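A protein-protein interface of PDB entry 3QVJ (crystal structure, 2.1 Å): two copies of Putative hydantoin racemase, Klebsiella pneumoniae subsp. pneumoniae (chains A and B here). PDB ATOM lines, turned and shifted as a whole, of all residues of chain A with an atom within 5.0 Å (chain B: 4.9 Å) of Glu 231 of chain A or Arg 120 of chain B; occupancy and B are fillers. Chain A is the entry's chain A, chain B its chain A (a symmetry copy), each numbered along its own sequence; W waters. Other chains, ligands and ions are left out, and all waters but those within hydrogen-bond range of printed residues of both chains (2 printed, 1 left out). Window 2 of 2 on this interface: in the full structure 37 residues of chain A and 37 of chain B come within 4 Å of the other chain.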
ATOM      1  N   GLU A  88     -26.134 -23.357   4.390  1.00  0.00           N
ATOM      2  CA  GLU A  88     -26.549 -24.619   3.772  1.00  0.00           C
ATOM      3  C   GLU A  88     -27.580 -25.352   4.624  1.00  0.00           C
ATOM      4  O   GLU A  88     -28.580 -25.856   4.099  1.00  0.00           O
ATOM      5  CB  GLU A  88     -25.352 -25.536   3.549  1.00  0.00           C
ATOM      6  CG  GLU A  88     -24.394 -25.059   2.472  1.00  0.00           C
ATOM      7  CD  GLU A  88     -23.317 -26.076   2.151  1.00  0.00           C
ATOM      8  OE1 GLU A  88     -23.245 -27.131   2.813  1.00  0.00           O
ATOM      9  OE2 GLU A  88     -22.550 -25.829   1.205  1.00  0.00           O
ATOM     10  N   GLY A 225     -28.133 -24.251  -5.831  1.00  0.00           N
ATOM     11  CA  GLY A 225     -26.685 -24.359  -6.018  1.00  0.00           C
ATOM     12  C   GLY A 225     -25.822 -24.380  -4.763  1.00  0.00           C
ATOM     13  O   GLY A 225     -25.917 -25.294  -3.944  1.00  0.00           O
ATOM     14  N   ASP A 226     -24.975 -23.363  -4.626  1.00  0.00           N
ATOM     15  CA  ASP A 226     -23.899 -23.347  -3.630  1.00  0.00           C
ATOM     16  C   ASP A 226     -24.348 -23.501  -2.181  1.00  0.00           C
ATOM     17  O   ASP A 226     -23.651 -24.121  -1.380  1.00  0.00           O
ATOM     18  CB  ASP A 226     -23.056 -22.072  -3.767  1.00  0.00           C
ATOM     19  CG  ASP A 226     -22.343 -21.983  -5.098  1.00  0.00           C
ATOM     20  OD1 ASP A 226     -22.330 -22.985  -5.854  1.00  0.00           O
ATOM     21  OD2 ASP A 226     -21.791 -20.902  -5.385  1.00  0.00           O
ATOM     22  N   LEU A 227     -25.496 -22.926  -1.847  1.00  0.00           N
ATOM     23  CA  LEU A 227     -25.973 -22.942  -0.473  1.00  0.00           C
ATOM     24  C   LEU A 227     -27.206 -23.836  -0.304  1.00  0.00           C
ATOM     25  O   LEU A 227     -27.989 -23.663   0.632  1.00  0.00           O
ATOM     26  CB  LEU A 227     -26.228 -21.512   0.022  1.00  0.00           C
ATOM     27  CG  LEU A 227     -25.039 -20.540  -0.006  1.00  0.00           C
ATOM     28  CD1 LEU A 227     -25.449 -19.172   0.509  1.00  0.00           C
ATOM     29  CD2 LEU A 227     -23.839 -21.078   0.785  1.00  0.00           C
ATOM     30  N   ALA A 228     -27.358 -24.796  -1.215  1.00  0.00           N
ATOM     31  CA  ALA A 228     -28.421 -25.789  -1.121  1.00  0.00           C
ATOM     32  C   ALA A 228     -28.219 -26.585   0.159  1.00  0.00           C
ATOM     33  O   ALA A 228     -27.118 -26.588   0.726  1.00  0.00           O
ATOM     34  CB  ALA A 228     -28.399 -26.713  -2.335  1.00  0.00           C
ATOM     35  N   PHE A 229     -29.280 -27.236   0.630  1.00  0.00           N
ATOM     36  CA  PHE A 229     -29.164 -28.134   1.775  1.00  0.00           C
ATOM     37  C   PHE A 229     -28.048 -29.138   1.494  1.00  0.00           C
ATOM     38  O   PHE A 229     -27.829 -29.508   0.335  1.00  0.00           O
ATOM     39  CB  PHE A 229     -30.500 -28.833   2.081  1.00  0.00           C
ATOM     40  CG  PHE A 229     -31.585 -27.888   2.553  1.00  0.00           C
ATOM     41  CD1 PHE A 229     -31.462 -27.210   3.767  1.00  0.00           C
ATOM     42  CD2 PHE A 229     -32.727 -27.675   1.782  1.00  0.00           C
ATOM     43  CE1 PHE A 229     -32.457 -26.330   4.207  1.00  0.00           C
ATOM     44  CE2 PHE A 229     -33.730 -26.800   2.207  1.00  0.00           C
ATOM     45  CZ  PHE A 229     -33.597 -26.123   3.427  1.00  0.00           C
ATOM     46  N   PRO A 230     -27.303 -29.546   2.538  1.00  0.00           N
ATOM     47  CA  PRO A 230     -26.215 -30.506   2.329  1.00  0.00           C
ATOM     48  C   PRO A 230     -26.705 -31.770   1.616  1.00  0.00           C
ATOM     49  O   PRO A 230     -27.853 -32.160   1.792  1.00  0.00           O
ATOM     50  CB  PRO A 230     -25.764 -30.846   3.757  1.00  0.00           C
ATOM     51  CG  PRO A 230     -26.170 -29.669   4.573  1.00  0.00           C
ATOM     52  CD  PRO A 230     -27.427 -29.141   3.951  1.00  0.00           C
ATOM     53  N   GLU A 231     -25.850 -32.388   0.803  1.00  0.00           N
ATOM     54  CA  GLU A 231     -26.171 -33.693   0.214  1.00  0.00           C
ATOM     55  C   GLU A 231     -26.462 -34.676   1.355  1.00  0.00           C
ATOM     56  O   GLU A 231     -25.771 -34.660   2.383  1.00  0.00           O
ATOM     57  CB  GLU A 231     -25.025 -34.212  -0.668  1.00  0.00           C
ATOM     58  CG  GLU A 231     -24.473 -33.210  -1.704  1.00  0.00           C
ATOM     59  CD  GLU A 231     -25.504 -32.779  -2.744  1.00  0.00           C
ATOM     60  OE1 GLU A 231     -26.190 -33.660  -3.305  1.00  0.00           O
ATOM     61  OE2 GLU A 231     -25.626 -31.561  -3.006  1.00  0.00           O
ATOM     62  N   LYS A 232     -27.505 -35.490   1.192  1.00  0.00           N
ATOM     63  CA  LYS A 232     -27.927 -36.432   2.233  1.00  0.00           C
ATOM     64  C   LYS A 232     -26.838 -37.482   2.473  1.00  0.00           C
ATOM     65  O   LYS A 232     -26.511 -38.259   1.579  1.00  0.00           O
ATOM     66  CB  LYS A 232     -29.258 -37.098   1.854  1.00  0.00           C
ATOM     67  CG  LYS A 232     -29.854 -37.987   2.936  1.00  0.00           C
ATOM     68  N   LYS A 233     -26.272 -37.482   3.678  1.00  0.00           N
ATOM     69  CA  LYS A 233     -25.145 -38.357   4.014  1.00  0.00           C
ATOM     70  C   LYS A 233     -25.251 -38.896   5.427  1.00  0.00           C
ATOM     71  O   LYS A 233     -25.806 -38.242   6.306  1.00  0.00           O
ATOM     72  CB  LYS A 233     -23.817 -37.607   3.869  1.00  0.00           C
ATOM     73  CG  LYS A 233     -23.328 -37.498   2.446  1.00  0.00           C
ATOM     74  CD  LYS A 233     -22.269 -36.428   2.321  1.00  0.00           C
ATOM     75  CE  LYS A 233     -21.923 -36.197   0.874  1.00  0.00           C
ATOM     76  NZ  LYS A 233     -20.994 -35.051   0.716  1.00  0.00           N
ATOM     77  N   ASN A 243     -27.716 -33.306  11.100  1.00  0.00           N
ATOM     78  CA  ASN A 243     -28.622 -33.163   9.962  1.00  0.00           C
ATOM     79  C   ASN A 243     -29.707 -34.248   9.918  1.00  0.00           C
ATOM     80  O   ASN A 243     -29.680 -35.119   9.045  1.00  0.00           O
ATOM     81  CB  ASN A 243     -27.820 -33.115   8.648  1.00  0.00           C
ATOM     82  CG  ASN A 243     -28.651 -32.653   7.455  1.00  0.00           C
ATOM     83  OD1 ASN A 243     -29.739 -32.087   7.607  1.00  0.00           O
ATOM     84  ND2 ASN A 243     -28.133 -32.894   6.255  1.00  0.00           N
ATOM     85  N   GLU B  46     -18.533 -32.503   0.022  1.00  0.00           N
ATOM     86  CA  GLU B  46     -19.125 -31.846  -1.151  1.00  0.00           C
ATOM     87  C   GLU B  46     -19.945 -30.625  -0.753  1.00  0.00           C
ATOM     88  O   GLU B  46     -21.148 -30.569  -1.012  1.00  0.00           O
ATOM     89  CB  GLU B  46     -20.039 -32.818  -1.901  1.00  0.00           C
ATOM     90  CG  GLU B  46     -19.386 -34.119  -2.337  1.00  0.00           C
ATOM     91  CD  GLU B  46     -20.394 -35.180  -2.691  1.00  0.00           C
ATOM     92  OE1 GLU B  46     -21.454 -35.251  -2.036  1.00  0.00           O
ATOM     93  OE2 GLU B  46     -20.120 -35.952  -3.627  1.00  0.00           O
ATOM     94  N   GLY B  47     -19.305 -29.650  -0.124  1.00  0.00           N
ATOM     95  CA  GLY B  47     -20.009 -28.453   0.325  1.00  0.00           C
ATOM     96  C   GLY B  47     -19.497 -27.945   1.654  1.00  0.00           C
ATOM     97  O   GLY B  47     -18.641 -28.577   2.283  1.00  0.00           O
ATOM     98  N   LEU B 118     -18.616 -32.018  -8.167  1.00  0.00           N
ATOM     99  CA  LEU B 118     -19.953 -31.443  -8.284  1.00  0.00           C
ATOM    100  C   LEU B 118     -19.872 -29.937  -8.513  1.00  0.00           C
ATOM    101  O   LEU B 118     -18.904 -29.306  -8.081  1.00  0.00           O
ATOM    102  CB  LEU B 118     -20.767 -31.735  -7.017  1.00  0.00           C
ATOM    103  CG  LEU B 118     -21.233 -33.168  -6.746  1.00  0.00           C
ATOM    104  CD1 LEU B 118     -21.842 -33.249  -5.358  1.00  0.00           C
ATOM    105  CD2 LEU B 118     -22.240 -33.661  -7.801  1.00  0.00           C
ATOM    106  N   PRO B 119     -20.876 -29.357  -9.205  1.00  0.00           N
ATOM    107  CA  PRO B 119     -20.936 -27.897  -9.382  1.00  0.00           C
ATOM    108  C   PRO B 119     -20.813 -27.082  -8.087  1.00  0.00           C
ATOM    109  O   PRO B 119     -20.202 -26.012  -8.101  1.00  0.00           O
ATOM    110  CB  PRO B 119     -22.314 -27.680 -10.024  1.00  0.00           C
ATOM    111  CG  PRO B 119     -22.546 -28.916 -10.820  1.00  0.00           C
ATOM    112  CD  PRO B 119     -21.871 -30.048 -10.053  1.00  0.00           C
ATOM    113  N   ARG B 120     -21.373 -27.583  -6.985  1.00  0.00           N
ATOM    114  CA  ARG B 120     -21.390 -26.830  -5.723  1.00  0.00           C
ATOM    115  C   ARG B 120     -20.021 -26.718  -5.035  1.00  0.00           C
ATOM    116  O   ARG B 120     -19.860 -25.945  -4.090  1.00  0.00           O
ATOM    117  CB  ARG B 120     -22.444 -27.382  -4.754  1.00  0.00           C
ATOM    118  CG  ARG B 120     -22.102 -28.724  -4.113  1.00  0.00           C
ATOM    119  CD  ARG B 120     -23.180 -29.166  -3.116  1.00  0.00           C
ATOM    120  NE  ARG B 120     -23.475 -28.133  -2.123  1.00  0.00           N
ATOM    121  CZ  ARG B 120     -24.521 -28.151  -1.296  1.00  0.00           C
ATOM    122  NH1 ARG B 120     -25.389 -29.161  -1.313  1.00  0.00           N
ATOM    123  NH2 ARG B 120     -24.703 -27.157  -0.443  1.00  0.00           N
ATOM    124  N   THR B 121     -19.049 -27.488  -5.516  1.00  0.00           N
ATOM    125  CA  THR B 121     -17.691 -27.427  -4.993  1.00  0.00           C
ATOM    126  C   THR B 121     -16.844 -26.389  -5.745  1.00  0.00           C
ATOM    127  O   THR B 121     -15.750 -26.049  -5.301  1.00  0.00           O
ATOM    128  CB  THR B 121     -16.981 -28.805  -5.046  1.00  0.00           C
ATOM    129  OG1 THR B 121     -16.709 -29.160  -6.407  1.00  0.00           O
ATOM    130  CG2 THR B 121     -17.842 -29.894  -4.386  1.00  0.00           C
ATOM    131  N   LEU B 122     -17.349 -25.902  -6.878  1.00  0.00           N
ATOM    132  CA  LEU B 122     -16.628 -24.898  -7.673  1.00  0.00           C
ATOM    133  C   LEU B 122     -16.354 -23.628  -6.869  1.00  0.00           C
ATOM    134  O   LEU B 122     -15.235 -23.128  -6.879  1.00  0.00           O
ATOM    135  CB  LEU B 122     -17.366 -24.569  -8.979  1.00  0.00           C
ATOM    136  CG  LEU B 122     -17.412 -25.652 -10.068  1.00  0.00           C
ATOM    137  CD1 LEU B 122     -18.408 -25.290 -11.168  1.00  0.00           C
ATOM    138  CD2 LEU B 122     -16.038 -25.907 -10.667  1.00  0.00           C
ATOM    139  N   ILE B 123     -17.368 -23.138  -6.154  1.00  0.00           N
ATOM    140  CA  ILE B 123     -17.231 -21.949  -5.298  1.00  0.00           C
ATOM    141  C   ILE B 123     -16.195 -22.163  -4.181  1.00  0.00           C
ATOM    142  O   ILE B 123     -15.521 -21.220  -3.771  1.00  0.00           O
ATOM    143  CB  ILE B 123     -18.609 -21.464  -4.719  1.00  0.00           C
ATOM    144  CG1 ILE B 123     -18.526 -20.026  -4.168  1.00  0.00           C
ATOM    145  CG2 ILE B 123     -19.136 -22.424  -3.647  1.00  0.00           C
ATOM    146  CD1 ILE B 123     -18.274 -18.948  -5.235  1.00  0.00           C
ATOM    147  N   ILE B 124     -16.062 -23.402  -3.708  1.00  0.00           N
ATOM    148  CA  ILE B 124     -15.047 -23.733  -2.705  1.00  0.00           C
ATOM    149  C   ILE B 124     -13.657 -23.598  -3.331  1.00  0.00           C
ATOM    150  O   ILE B 124     -12.768 -22.985  -2.745  1.00  0.00           O
ATOM    151  CB  ILE B 124     -15.222 -25.157  -2.133  1.00  0.00           C
ATOM    152  CG1 ILE B 124     -16.646 -25.361  -1.590  1.00  0.00           C
ATOM    153  CG2 ILE B 124     -14.140 -25.453  -1.067  1.00  0.00           C
ATOM    154  CD1 ILE B 124     -16.791 -25.137  -0.107  1.00  0.00           C
HETATM  155  O   HOH W   1     -22.927 -31.586   0.840  1.00  0.00           O
HETATM  156  O   HOH W   2     -20.078 -23.469  -7.234  1.00  0.00           O
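Glu 231 of chain A touches two residues of chain B.
Of the printed residues of chain B, Asp 226 of chain A touches Arg 120 (3.3 Å) and Ile 123 (3.3 Å).
Printed residues of chain B within 4 Å of Pro 230 of chain A: Arg 120.
Printed residues of chain A within 4 Å of Gly 47 of chain B: Glu 88 (3.7 Å).
Printed residues of chain B within 4 Å of Glu 88 of chain A: Gly 47 (3.7 Å) and Arg 120 (3.0 Å).
Of the printed residues of chain B, Phe 229 of chain A touches Arg 120.
Lys 232 of chain A touches none of the printed residues of chain B.
Thr 121 of chain B touches none of the printed residues of chain A.
The nearest residue of chain B that does not touch Glu 231 of chain A is Leu 118 of chain B (4.5 Å).
The nearest printed residue of chain A that does not touch Arg 120 of chain B is Gly 225 of chain A (4.1 Å).
The nearest printed residue of chain B that does not touch Glu 88 of chain A is Glu 46 of chain B (5.4 Å).
No position is printed for both chains.
Of the 10 pairs that touch across the chains among the printed residues, none has its exchanged pair printed and touching as well.
Of the 9 printed residues of chain B, 4 touch a printed residue of chain A.
Printed residues of chain B that touch a printed residue of chain A: Glu 46, Gly 47, Arg 120 and Ile 123.
Hydrophobic or aromatic side chains of chain B within 4 Å of the printed part of chain A: Ile 123.
Along chain B the printed residues that touch a printed residue of chain A span positions 46 to 123.
Along chain A the printed residues that touch a printed residue of chain B span positions 88 to 233.
Among the printed residues, 10 pairs touch across the chains.
The guanidinium group (NH1) of Arg 120 of chain B is in salt-bridge range of the side-chain carboxylate (OE2) of Glu 231 of chain A (2.9 Å).
The side-chain carboxylate (OE2) of Glu 88 of chain A is in salt-bridge range of the guanidinium group (NH2) of Arg 120 of chain B (3.0 Å).
The side-chain amino group (NZ) of Lys 233 of chain A lies within salt-bridge range of the side-chain carboxylate (OE1) of Glu 46 of chain B, 2.8 Å away.
The backbone carbonyl oxygen (O) of Ala 228 of chain A is in hydrogen-bond range of the guanidinium group (NH2) of Arg 120 of chain B (2.7 Å).
The guanidinium group of Arg 120 of chain B is in hydrogen-bond range of the backbone carbonyl oxygen of Phe 229 of chain A (3.0 Å).
NH2 of Arg 120 of chain B lies within hydrogen-bond range of O of Asp 226 of chain A (3.3 Å).
Water W2 lies within hydrogen-bond range of OD1 of Asp 226 of chain A (2.7 Å), O of Pro 119 of chain B (2.7 Å) and N of Ile 123 of chain B (2.9 Å).
Water W1 bridges O of Glu 46 of chain B and N of Glu 231 of chain A.
Among the printed residues, pairs that only touch across the chains: Glu 88 of chain A with Gly 47 of chain B, Asp 226 of chain A with Ile 123 of chain B, Pro 230 of chain A with Arg 120 of chain B and Glu 231 of chain A with Glu 46 of chain B.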
